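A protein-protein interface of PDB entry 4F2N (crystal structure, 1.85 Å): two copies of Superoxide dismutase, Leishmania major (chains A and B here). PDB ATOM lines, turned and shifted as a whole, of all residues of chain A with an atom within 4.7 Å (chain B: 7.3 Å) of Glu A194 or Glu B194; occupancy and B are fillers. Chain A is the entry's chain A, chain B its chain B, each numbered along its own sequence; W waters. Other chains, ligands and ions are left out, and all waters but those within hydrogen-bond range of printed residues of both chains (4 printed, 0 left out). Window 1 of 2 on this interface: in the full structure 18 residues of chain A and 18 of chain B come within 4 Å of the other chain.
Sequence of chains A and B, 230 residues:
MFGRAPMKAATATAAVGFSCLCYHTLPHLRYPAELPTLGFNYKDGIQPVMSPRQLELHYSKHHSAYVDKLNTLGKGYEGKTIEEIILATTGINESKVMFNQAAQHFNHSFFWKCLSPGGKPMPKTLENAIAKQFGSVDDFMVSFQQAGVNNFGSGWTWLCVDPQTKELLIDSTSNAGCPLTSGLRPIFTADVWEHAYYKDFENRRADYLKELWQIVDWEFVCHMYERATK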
ATOM      1  N   HIS A  62      -7.546  -6.275   7.486  1.00  0.00           N
ATOM      2  CA  HIS A  62      -8.242  -7.545   7.669  1.00  0.00           C
ATOM      3  C   HIS A  62      -9.262  -7.776   6.582  1.00  0.00           C
ATOM      4  O   HIS A  62      -9.151  -8.760   5.827  1.00  0.00           O
ATOM      5  CB  HIS A  62      -8.855  -7.649   9.079  1.00  0.00           C
ATOM      6  CG  HIS A  62      -7.836  -7.690  10.180  1.00  0.00           C
ATOM      7  ND1 HIS A  62      -7.165  -8.814  10.520  1.00  0.00           N
ATOM      8  CD2 HIS A  62      -7.336  -6.681  10.995  1.00  0.00           C
ATOM      9  CE1 HIS A  62      -6.324  -8.538  11.533  1.00  0.00           C
ATOM     10  NE2 HIS A  62      -6.424  -7.239  11.815  1.00  0.00           N
ATOM     11  N   VAL A 192     -16.233 -10.739  17.219  1.00  0.00           N
ATOM     12  CA  VAL A 192     -15.453 -10.931  18.454  1.00  0.00           C
ATOM     13  C   VAL A 192     -14.100 -11.603  18.184  1.00  0.00           C
ATOM     14  O   VAL A 192     -13.436 -12.071  19.113  1.00  0.00           O
ATOM     15  CB  VAL A 192     -16.256 -11.650  19.592  1.00  0.00           C
ATOM     16  CG1 VAL A 192     -17.439 -10.796  20.071  1.00  0.00           C
ATOM     17  CG2 VAL A 192     -16.749 -13.024  19.140  1.00  0.00           C
ATOM     18  N   TRP A 193     -13.676 -11.661  16.917  1.00  0.00           N
ATOM     19  CA  TRP A 193     -12.232 -11.792  16.677  1.00  0.00           C
ATOM     20  C   TRP A 193     -11.553 -10.704  17.459  1.00  0.00           C
ATOM     21  O   TRP A 193     -12.045  -9.587  17.504  1.00  0.00           O
ATOM     22  CB  TRP A 193     -11.890 -11.621  15.222  1.00  0.00           C
ATOM     23  CG  TRP A 193     -12.275 -12.805  14.335  1.00  0.00           C
ATOM     24  CD1 TRP A 193     -13.544 -13.346  14.105  1.00  0.00           C
ATOM     25  CD2 TRP A 193     -11.363 -13.564  13.474  1.00  0.00           C
ATOM     26  NE1 TRP A 193     -13.474 -14.399  13.213  1.00  0.00           N
ATOM     27  CE2 TRP A 193     -12.185 -14.564  12.779  1.00  0.00           C
ATOM     28  CE3 TRP A 193      -9.987 -13.523  13.241  1.00  0.00           C
ATOM     29  CZ2 TRP A 193     -11.629 -15.484  11.891  1.00  0.00           C
ATOM     30  CZ3 TRP A 193      -9.436 -14.430  12.318  1.00  0.00           C
ATOM     31  CH2 TRP A 193     -10.246 -15.392  11.661  1.00  0.00           C
ATOM     32  N   GLU A 194     -10.442 -11.044  18.114  1.00  0.00           N
ATOM     33  CA  GLU A 194      -9.674 -10.080  18.927  1.00  0.00           C
ATOM     34  C   GLU A 194      -9.271  -8.846  18.157  1.00  0.00           C
ATOM     35  O   GLU A 194      -9.302  -7.763  18.733  1.00  0.00           O
ATOM     36  CB  GLU A 194      -8.467 -10.761  19.599  1.00  0.00           C
ATOM     37  CG  GLU A 194      -8.965 -11.904  20.503  1.00  0.00           C
ATOM     38  CD  GLU A 194      -7.847 -12.643  21.233  1.00  0.00           C
ATOM     39  OE1 GLU A 194      -6.866 -13.046  20.575  1.00  0.00           O
ATOM     40  OE2 GLU A 194      -7.977 -12.844  22.464  1.00  0.00           O
ATOM     41  N   HIS A 195      -8.931  -8.989  16.871  1.00  0.00           N
ATOM     42  CA  HIS A 195      -8.605  -7.798  16.044  1.00  0.00           C
ATOM     43  C   HIS A 195      -9.719  -6.771  15.967  1.00  0.00           C
ATOM     44  O   HIS A 195      -9.447  -5.652  15.652  1.00  0.00           O
ATOM     45  CB  HIS A 195      -8.122  -8.169  14.636  1.00  0.00           C
ATOM     46  CG  HIS A 195      -9.203  -8.757  13.741  1.00  0.00           C
ATOM     47  ND1 HIS A 195      -9.093  -9.983  13.202  1.00  0.00           N
ATOM     48  CD2 HIS A 195     -10.395  -8.221  13.263  1.00  0.00           C
ATOM     49  CE1 HIS A 195     -10.166 -10.250  12.443  1.00  0.00           C
ATOM     50  NE2 HIS A 195     -10.967  -9.173  12.458  1.00  0.00           N
ATOM     51  N   ALA A 196     -10.982  -7.157  16.219  1.00  0.00           N
ATOM     52  CA  ALA A 196     -12.125  -6.216  16.133  1.00  0.00           C
ATOM     53  C   ALA A 196     -12.051  -5.138  17.229  1.00  0.00           C
ATOM     54  O   ALA A 196     -12.527  -3.981  17.052  1.00  0.00           O
ATOM     55  CB  ALA A 196     -13.465  -7.002  16.274  1.00  0.00           C
ATOM     56  N   TYR A 197     -11.466  -5.511  18.360  1.00  0.00           N
ATOM     57  CA  TYR A 197     -11.444  -4.610  19.510  1.00  0.00           C
ATOM     58  C   TYR A 197     -10.084  -4.364  20.162  1.00  0.00           C
ATOM     59  O   TYR A 197      -9.996  -3.496  21.040  1.00  0.00           O
ATOM     60  CB  TYR A 197     -12.421  -5.114  20.583  1.00  0.00           C
ATOM     61  CG  TYR A 197     -12.115  -6.525  21.052  1.00  0.00           C
ATOM     62  CD1 TYR A 197     -11.172  -6.760  22.060  1.00  0.00           C
ATOM     63  CD2 TYR A 197     -12.834  -7.615  20.548  1.00  0.00           C
ATOM     64  CE1 TYR A 197     -10.906  -8.037  22.509  1.00  0.00           C
ATOM     65  CE2 TYR A 197     -12.566  -8.905  20.986  1.00  0.00           C
ATOM     66  CZ  TYR A 197     -11.635  -9.101  21.980  1.00  0.00           C
ATOM     67  OH  TYR A 197     -11.390 -10.381  22.414  1.00  0.00           O
ATOM     68  N   TYR A 198      -9.035  -5.108  19.785  1.00  0.00           N
ATOM     69  CA  TYR A 198      -7.776  -5.053  20.566  1.00  0.00           C
ATOM     70  C   TYR A 198      -7.078  -3.703  20.542  1.00  0.00           C
ATOM     71  O   TYR A 198      -6.409  -3.335  21.525  1.00  0.00           O
ATOM     72  CB  TYR A 198      -6.779  -6.136  20.119  1.00  0.00           C
ATOM     73  CG  TYR A 198      -6.085  -6.750  21.279  1.00  0.00           C
ATOM     74  CD1 TYR A 198      -6.721  -7.717  22.031  1.00  0.00           C
ATOM     75  CD2 TYR A 198      -4.795  -6.316  21.668  1.00  0.00           C
ATOM     76  CE1 TYR A 198      -6.112  -8.260  23.138  1.00  0.00           C
ATOM     77  CE2 TYR A 198      -4.164  -6.880  22.763  1.00  0.00           C
ATOM     78  CZ  TYR A 198      -4.845  -7.855  23.499  1.00  0.00           C
ATOM     79  OH  TYR A 198      -4.267  -8.440  24.608  1.00  0.00           O
ATOM     80  N   ARG A 205     -12.723  -7.461  26.026  1.00  0.00           N
ATOM     81  CA  ARG A 205     -13.823  -7.827  25.126  1.00  0.00           C
ATOM     82  C   ARG A 205     -15.190  -7.497  25.755  1.00  0.00           C
ATOM     83  O   ARG A 205     -16.067  -6.972  25.070  1.00  0.00           O
ATOM     84  CB  ARG A 205     -13.810  -9.325  24.770  1.00  0.00           C
ATOM     85  CG  ARG A 205     -14.892  -9.713  23.747  1.00  0.00           C
ATOM     86  CD  ARG A 205     -15.120 -11.227  23.624  1.00  0.00           C
ATOM     87  NE  ARG A 205     -14.026 -11.842  22.859  1.00  0.00           N
ATOM     88  CZ  ARG A 205     -14.018 -13.085  22.386  1.00  0.00           C
ATOM     89  NH1 ARG A 205     -15.063 -13.909  22.579  1.00  0.00           N
ATOM     90  NH2 ARG A 205     -12.962 -13.523  21.701  1.00  0.00           N
ATOM     91  N   GLN B  54       2.779  -5.482  25.886  1.00  0.00           N
ATOM     92  CA  GLN B  54       2.323  -6.736  25.220  1.00  0.00           C
ATOM     93  C   GLN B  54       2.421  -7.917  26.174  1.00  0.00           C
ATOM     94  O   GLN B  54       1.496  -8.764  26.249  1.00  0.00           O
ATOM     95  CB  GLN B  54       3.142  -7.007  23.947  1.00  0.00           C
ATOM     96  CG  GLN B  54       2.874  -8.330  23.252  1.00  0.00           C
ATOM     97  CD  GLN B  54       1.514  -8.359  22.560  1.00  0.00           C
ATOM     98  OE1 GLN B  54       1.394  -8.031  21.369  1.00  0.00           O
ATOM     99  NE2 GLN B  54       0.479  -8.727  23.311  1.00  0.00           N
ATOM    100  N   HIS B  62      -4.614 -12.176  30.088  1.00  0.00           N
ATOM    101  CA  HIS B  62      -5.089 -13.400  29.407  1.00  0.00           C
ATOM    102  C   HIS B  62      -4.773 -14.663  30.168  1.00  0.00           C
ATOM    103  O   HIS B  62      -5.664 -15.428  30.542  1.00  0.00           O
ATOM    104  CB  HIS B  62      -4.530 -13.486  27.987  1.00  0.00           C
ATOM    105  CG  HIS B  62      -5.072 -12.421  27.063  1.00  0.00           C
ATOM    106  ND1 HIS B  62      -6.212 -12.579  26.365  1.00  0.00           N
ATOM    107  CD2 HIS B  62      -4.575 -11.172  26.725  1.00  0.00           C
ATOM    108  CE1 HIS B  62      -6.445 -11.476  25.629  1.00  0.00           C
ATOM    109  NE2 HIS B  62      -5.428 -10.617  25.845  1.00  0.00           N
ATOM    110  N   TYR B  66      -7.282 -17.434  32.637  1.00  0.00           N
ATOM    111  CA  TYR B  66      -7.409 -18.904  32.503  1.00  0.00           C
ATOM    112  C   TYR B  66      -7.102 -19.604  33.834  1.00  0.00           C
ATOM    113  O   TYR B  66      -7.772 -20.561  34.215  1.00  0.00           O
ATOM    114  CB  TYR B  66      -6.434 -19.439  31.434  1.00  0.00           C
ATOM    115  CG  TYR B  66      -6.753 -18.975  30.027  1.00  0.00           C
ATOM    116  CD1 TYR B  66      -7.978 -19.298  29.426  1.00  0.00           C
ATOM    117  CD2 TYR B  66      -5.828 -18.247  29.288  1.00  0.00           C
ATOM    118  CE1 TYR B  66      -8.283 -18.892  28.122  1.00  0.00           C
ATOM    119  CE2 TYR B  66      -6.117 -17.835  27.995  1.00  0.00           C
ATOM    120  CZ  TYR B  66      -7.345 -18.172  27.413  1.00  0.00           C
ATOM    121  OH  TYR B  66      -7.607 -17.774  26.127  1.00  0.00           O
ATOM    122  N   GLY B 153      -7.830 -18.274  12.231  1.00  0.00           N
ATOM    123  CA  GLY B 153      -8.458 -17.938  13.539  1.00  0.00           C
ATOM    124  C   GLY B 153      -7.431 -17.954  14.654  1.00  0.00           C
ATOM    125  O   GLY B 153      -6.221 -17.636  14.429  1.00  0.00           O
ATOM    126  N   SER B 154      -7.877 -18.326  15.850  1.00  0.00           N
ATOM    127  CA  SER B 154      -6.964 -18.410  17.006  1.00  0.00           C
ATOM    128  C   SER B 154      -6.328 -19.784  17.089  1.00  0.00           C
ATOM    129  O   SER B 154      -6.979 -20.798  16.759  1.00  0.00           O
ATOM    130  CB  SER B 154      -7.729 -18.170  18.310  1.00  0.00           C
ATOM    131  OG  SER B 154      -8.541 -17.001  18.225  1.00  0.00           O
ATOM    132  N   GLY B 155      -5.102 -19.857  17.567  1.00  0.00           N
ATOM    133  CA  GLY B 155      -4.550 -21.181  17.924  1.00  0.00           C
ATOM    134  C   GLY B 155      -3.067 -21.132  18.194  1.00  0.00           C
ATOM    135  O   GLY B 155      -2.527 -20.078  18.535  1.00  0.00           O
ATOM    136  N   ASP B 191       2.279 -19.052  20.140  1.00  0.00           N
ATOM    137  CA  ASP B 191       0.864 -18.661  20.269  1.00  0.00           C
ATOM    138  C   ASP B 191       0.505 -17.802  19.051  1.00  0.00           C
ATOM    139  O   ASP B 191       1.195 -16.803  18.785  1.00  0.00           O
ATOM    140  CB  ASP B 191       0.734 -17.802  21.546  1.00  0.00           C
ATOM    141  CG  ASP B 191      -0.701 -17.511  21.941  1.00  0.00           C
ATOM    142  OD1 ASP B 191      -1.643 -17.929  21.222  1.00  0.00           O
ATOM    143  OD2 ASP B 191      -0.901 -16.880  23.027  1.00  0.00           O
ATOM    144  N   VAL B 192      -0.519 -18.188  18.287  1.00  0.00           N
ATOM    145  CA  VAL B 192      -0.979 -17.315  17.206  1.00  0.00           C
ATOM    146  C   VAL B 192      -2.437 -16.874  17.388  1.00  0.00           C
ATOM    147  O   VAL B 192      -3.094 -16.432  16.440  1.00  0.00           O
ATOM    148  CB  VAL B 192      -0.715 -17.871  15.792  1.00  0.00           C
ATOM    149  CG1 VAL B 192       0.780 -17.999  15.525  1.00  0.00           C
ATOM    150  CG2 VAL B 192      -1.350 -19.242  15.663  1.00  0.00           C
ATOM    151  N   TRP B 193      -2.953 -16.945  18.622  1.00  0.00           N
ATOM    152  CA  TRP B 193      -4.095 -16.079  18.964  1.00  0.00           C
ATOM    153  C   TRP B 193      -3.684 -14.675  18.678  1.00  0.00           C
ATOM    154  O   TRP B 193      -2.514 -14.304  18.941  1.00  0.00           O
ATOM    155  CB  TRP B 193      -4.429 -16.204  20.446  1.00  0.00           C
ATOM    156  CG  TRP B 193      -5.215 -17.463  20.803  1.00  0.00           C
ATOM    157  CD1 TRP B 193      -4.812 -18.786  20.681  1.00  0.00           C
ATOM    158  CD2 TRP B 193      -6.500 -17.498  21.473  1.00  0.00           C
ATOM    159  NE1 TRP B 193      -5.784 -19.651  21.170  1.00  0.00           N
ATOM    160  CE2 TRP B 193      -6.835 -18.924  21.666  1.00  0.00           C
ATOM    161  CE3 TRP B 193      -7.416 -16.513  21.899  1.00  0.00           C
ATOM    162  CZ2 TRP B 193      -8.038 -19.324  22.259  1.00  0.00           C
ATOM    163  CZ3 TRP B 193      -8.626 -16.934  22.501  1.00  0.00           C
ATOM    164  CH2 TRP B 193      -8.920 -18.307  22.681  1.00  0.00           C
ATOM    165  N   GLU B 194      -4.618 -13.844  18.198  1.00  0.00           N
ATOM    166  CA  GLU B 194      -4.262 -12.483  17.790  1.00  0.00           C
ATOM    167  C   GLU B 194      -3.752 -11.660  18.957  1.00  0.00           C
ATOM    168  O   GLU B 194      -2.895 -10.781  18.777  1.00  0.00           O
ATOM    169  CB  GLU B 194      -5.435 -11.766  17.099  1.00  0.00           C
ATOM    170  CG  GLU B 194      -5.770 -12.369  15.741  1.00  0.00           C
ATOM    171  CD  GLU B 194      -6.945 -11.680  15.044  1.00  0.00           C
ATOM    172  OE1 GLU B 194      -8.045 -11.567  15.659  1.00  0.00           O
ATOM    173  OE2 GLU B 194      -6.765 -11.299  13.849  1.00  0.00           O
ATOM    174  N   HIS B 195      -4.251 -11.945  20.159  1.00  0.00           N
ATOM    175  CA  HIS B 195      -3.743 -11.247  21.347  1.00  0.00           C
ATOM    176  C   HIS B 195      -2.274 -11.485  21.612  1.00  0.00           C
ATOM    177  O   HIS B 195      -1.666 -10.689  22.345  1.00  0.00           O
ATOM    178  CB  HIS B 195      -4.584 -11.567  22.617  1.00  0.00           C
ATOM    179  CG  HIS B 195      -4.379 -12.958  23.161  1.00  0.00           C
ATOM    180  ND1 HIS B 195      -5.402 -13.863  23.269  1.00  0.00           N
ATOM    181  CD2 HIS B 195      -3.222 -13.604  23.661  1.00  0.00           C
ATOM    182  CE1 HIS B 195      -4.925 -15.026  23.802  1.00  0.00           C
ATOM    183  NE2 HIS B 195      -3.588 -14.872  24.028  1.00  0.00           N
ATOM    184  N   ALA B 196      -1.671 -12.547  21.053  1.00  0.00           N
ATOM    185  CA  ALA B 196      -0.244 -12.803  21.353  1.00  0.00           C
ATOM    186  C   ALA B 196       0.624 -11.714  20.741  1.00  0.00           C
ATOM    187  O   ALA B 196       1.719 -11.393  21.265  1.00  0.00           O
ATOM    188  CB  ALA B 196       0.202 -14.186  20.869  1.00  0.00           C
ATOM    189  N   TYR B 197       0.155 -11.120  19.649  1.00  0.00           N
ATOM    190  CA  TYR B 197       1.018 -10.187  18.896  1.00  0.00           C
ATOM    191  C   TYR B 197       0.353  -8.881  18.531  1.00  0.00           C
ATOM    192  O   TYR B 197       1.015  -8.032  17.935  1.00  0.00           O
ATOM    193  CB  TYR B 197       1.513 -10.858  17.588  1.00  0.00           C
ATOM    194  CG  TYR B 197       0.387 -11.332  16.673  1.00  0.00           C
ATOM    195  CD1 TYR B 197      -0.189 -10.477  15.716  1.00  0.00           C
ATOM    196  CD2 TYR B 197      -0.115 -12.628  16.772  1.00  0.00           C
ATOM    197  CE1 TYR B 197      -1.244 -10.931  14.893  1.00  0.00           C
ATOM    198  CE2 TYR B 197      -1.137 -13.080  15.954  1.00  0.00           C
ATOM    199  CZ  TYR B 197      -1.708 -12.222  15.034  1.00  0.00           C
ATOM    200  OH  TYR B 197      -2.726 -12.658  14.224  1.00  0.00           O
ATOM    201  N   TYR B 198      -0.939  -8.701  18.830  1.00  0.00           N
ATOM    202  CA  TYR B 198      -1.644  -7.535  18.253  1.00  0.00           C
ATOM    203  C   TYR B 198      -1.167  -6.190  18.801  1.00  0.00           C
ATOM    204  O   TYR B 198      -1.222  -5.176  18.093  1.00  0.00           O
ATOM    205  CB  TYR B 198      -3.173  -7.622  18.362  1.00  0.00           C
ATOM    206  CG  TYR B 198      -3.865  -7.076  17.125  1.00  0.00           C
ATOM    207  CD1 TYR B 198      -4.013  -7.865  15.992  1.00  0.00           C
ATOM    208  CD2 TYR B 198      -4.321  -5.760  17.078  1.00  0.00           C
ATOM    209  CE1 TYR B 198      -4.636  -7.376  14.844  1.00  0.00           C
ATOM    210  CE2 TYR B 198      -4.920  -5.237  15.930  1.00  0.00           C
ATOM    211  CZ  TYR B 198      -5.083  -6.053  14.821  1.00  0.00           C
ATOM    212  OH  TYR B 198      -5.690  -5.557  13.682  1.00  0.00           O
ATOM    213  N   LYS B 199      -0.760  -6.182  20.064  1.00  0.00           N
ATOM    214  CA  LYS B 199      -0.280  -4.929  20.680  1.00  0.00           C
ATOM    215  C   LYS B 199       0.940  -4.389  19.943  1.00  0.00           C
ATOM    216  O   LYS B 199       1.030  -3.194  19.690  1.00  0.00           O
ATOM    217  CB  LYS B 199       0.010  -5.118  22.179  1.00  0.00           C
ATOM    218  CG  LYS B 199       0.496  -3.857  22.903  1.00  0.00           C
ATOM    219  CD  LYS B 199      -0.642  -2.853  23.040  1.00  0.00           C
ATOM    220  CE  LYS B 199      -0.147  -1.526  23.598  1.00  0.00           C
ATOM    221  NZ  LYS B 199      -1.330  -0.657  23.844  1.00  0.00           N
ATOM    222  N   GLU B 202       0.147  -5.501  15.469  1.00  0.00           N
ATOM    223  CA  GLU B 202      -1.197  -5.359  14.888  1.00  0.00           C
ATOM    224  C   GLU B 202      -1.533  -6.603  14.026  1.00  0.00           C
ATOM    225  O   GLU B 202      -1.382  -7.742  14.497  1.00  0.00           O
ATOM    226  CB  GLU B 202      -1.311  -4.011  14.123  1.00  0.00           C
ATOM    227  CG  GLU B 202      -0.930  -2.816  15.018  1.00  0.00           C
ATOM    228  CD  GLU B 202      -0.874  -1.469  14.293  1.00  0.00           C
ATOM    229  OE1 GLU B 202      -0.427  -1.401  13.119  1.00  0.00           O
ATOM    230  OE2 GLU B 202      -1.265  -0.455  14.902  1.00  0.00           O
ATOM    231  N   ASN B 203      -1.966  -6.397  12.781  1.00  0.00           N
ATOM    232  CA  ASN B 203      -2.336  -7.473  11.875  1.00  0.00           C
ATOM    233  C   ASN B 203      -1.149  -8.271  11.352  1.00  0.00           C
ATOM    234  O   ASN B 203      -1.341  -9.242  10.641  1.00  0.00           O
ATOM    235  CB  ASN B 203      -3.086  -6.903  10.658  1.00  0.00           C
ATOM    236  CG  ASN B 203      -2.224  -5.951   9.861  1.00  0.00           C
ATOM    237  OD1 ASN B 203      -1.908  -4.899  10.343  1.00  0.00           O
ATOM    238  ND2 ASN B 203      -1.811  -6.343   8.660  1.00  0.00           N
ATOM    239  N   ARG B 205       0.907 -10.747  11.556  1.00  0.00           N
ATOM    240  CA  ARG B 205       1.244 -12.024  12.171  1.00  0.00           C
ATOM    241  C   ARG B 205       2.528 -12.614  11.569  1.00  0.00           C
ATOM    242  O   ARG B 205       3.327 -13.215  12.286  1.00  0.00           O
ATOM    243  CB  ARG B 205       0.081 -13.028  12.036  1.00  0.00           C
ATOM    244  CG  ARG B 205       0.334 -14.327  12.802  1.00  0.00           C
ATOM    245  CD  ARG B 205      -0.630 -15.444  12.463  1.00  0.00           C
ATOM    246  NE  ARG B 205      -1.973 -15.238  13.019  1.00  0.00           N
ATOM    247  CZ  ARG B 205      -2.960 -16.146  12.952  1.00  0.00           C
ATOM    248  NH1 ARG B 205      -2.752 -17.344  12.411  1.00  0.00           N
ATOM    249  NH2 ARG B 205      -4.160 -15.885  13.501  1.00  0.00           N
ATOM    250  N   TYR B 208       5.561 -11.019  13.131  1.00  0.00           N
ATOM    251  CA  TYR B 208       5.675 -11.530  14.498  1.00  0.00           C
ATOM    252  C   TYR B 208       6.396 -12.888  14.531  1.00  0.00           C
ATOM    253  O   TYR B 208       7.373 -13.053  15.253  1.00  0.00           O
ATOM    254  CB  TYR B 208       4.273 -11.631  15.127  1.00  0.00           C
ATOM    255  CG  TYR B 208       4.087 -12.657  16.250  1.00  0.00           C
ATOM    256  CD1 TYR B 208       4.755 -12.517  17.497  1.00  0.00           C
ATOM    257  CD2 TYR B 208       3.198 -13.722  16.090  1.00  0.00           C
ATOM    258  CE1 TYR B 208       4.564 -13.452  18.526  1.00  0.00           C
ATOM    259  CE2 TYR B 208       2.988 -14.644  17.105  1.00  0.00           C
ATOM    260  CZ  TYR B 208       3.644 -14.501  18.326  1.00  0.00           C
ATOM    261  OH  TYR B 208       3.423 -15.420  19.354  1.00  0.00           O
HETATM  262  O   HOH W   1      -1.940  -9.939  25.104  1.00  0.00           O
HETATM  263  O   HOH W   2      -7.288 -14.732  18.556  1.00  0.00           O
HETATM  264  O   HOH W   3      -8.411  -4.479  13.293  1.00  0.00           O
HETATM  265  O   HOH W   4      -9.209 -13.376  17.029  1.00  0.00           O
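NE2 of Gln B54 sits at hydrogen-bond distance from O of His B195 (3.1 Å).
A ring nitrogen (ND1) of His B62 sits at hydrogen-bond distance from a ring nitrogen (ND1) of His B195 (3.4 Å).
The guanidinium group of Arg B205 lies within hydrogen-bond range of the backbone carbonyl oxygen of Gly B153.
N of Trp B193 is in hydrogen-bond range of O of Gly B155.
The side-chain carboxylate (OD1) of Asp B191 sits at hydrogen-bond distance from the backbone NH (N) of Trp B193 (3.1 Å).
A ring nitrogen (NE2) of His A62 sits at hydrogen-bond distance from the side-chain hydroxyl of Tyr B198, 2.6 Å away.
The side-chain carboxylate (OE1) of Glu A194 lies within hydrogen-bond range of the backbone NH (N) of Glu B194.
OE1 of Glu A194 sits at hydrogen-bond distance from N of His B195.
A ring nitrogen (ND1) of His A195 is in hydrogen-bond range of the side-chain carboxylate (OE2) of Glu B194 (2.8 Å).
OH of Tyr A198 sits at hydrogen-bond distance from NE2 of His B62, 2.8 Å away.
Of the printed residues of chain B, His A62 touches Glu B194 (3.6 Å), Tyr B198 (2.6 Å) and Asn B203 (3.5 Å).
Of the printed residues of chain B, Trp A193 touches Gly B153 and Glu B194.
Of chain B, only His B62 (3.8 Å), Trp B193 (3.8 Å), Glu B194 (3.4 Å) and His B195 (2.9 Å) come within 4 Å of Glu A194.
Printed residues of chain B within 4 Å of Tyr A198: His B62, His B195 and Tyr B198.
Arg A205 touches none of the printed residues of chain B.
Printed residues of chain A within 4 Å of His B195: Glu A194 and Tyr A198.
Printed residues of chain A within 4 Å of Tyr B198: His A62, His A195 and Tyr A198.
Of the 9 printed residues of chain A, 5 touch a printed residue of chain B.
Along chain A the printed residues that touch a printed residue of chain B span positions 62 to 198.
Hydrophobic or aromatic side chains of chain B that line the printed part of chain A: His B62, Trp B193, His B195 and Tyr B198.
CE1 of His A62 touches OE2 of Glu B194 (3.6 Å).
His A62 touches Asn B203.
Gly B153 touches Trp A193 (CA to CH2, 3.6 Å).
Trp A193 touches Glu B194 (CE3 to OE1, 3.7 Å).
CE1 of His B62 touches OE2 of Glu A194, 3.8 Å away.
Glu A194 touches Trp B193 (OE1 to CE3, 3.8 Å).
His A195 touches Tyr B198 (CB to CE1, 3.6 Å).
CE1 of Tyr A198 touches CB of His B195 (3.7 Å).
CB of Tyr B198 touches CD2 of Tyr A198, at 3.9 Å.
Water W4 lies within hydrogen-bond range of OE1 of Glu B194 (2.6 Å) and N of Glu A194 (2.9 Å).
Water W2 lies within hydrogen-bond range of OG of Ser B154 (2.6 Å), OE1 of Glu A194 (2.7 Å) and N of Glu B194 (2.8 Å).
Water W1 lies within hydrogen-bond range of OH of Tyr A198 (2.8 Å), O of His B195 (2.9 Å) and NE2 of Gln B54 (3.2 Å).
Water W3 lies within hydrogen-bond range of the backbone carbonyl oxygen of His A195 (2.8 Å) and the side-chain hydroxyl of Tyr B198 (3.0 Å).
His A62 touches Tyr B198, and with the chains exchanged Tyr A198 touches His B62.
Trp A193 touches Glu B194, and with the chains exchanged Glu A194 touches Trp B193.
Glu A194 touches His B195, and with the chains exchanged His A195 touches Glu B194.
His A195 touches Tyr B198, and with the chains exchanged Tyr A198 touches His B195.
9 positions are printed for both chains.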
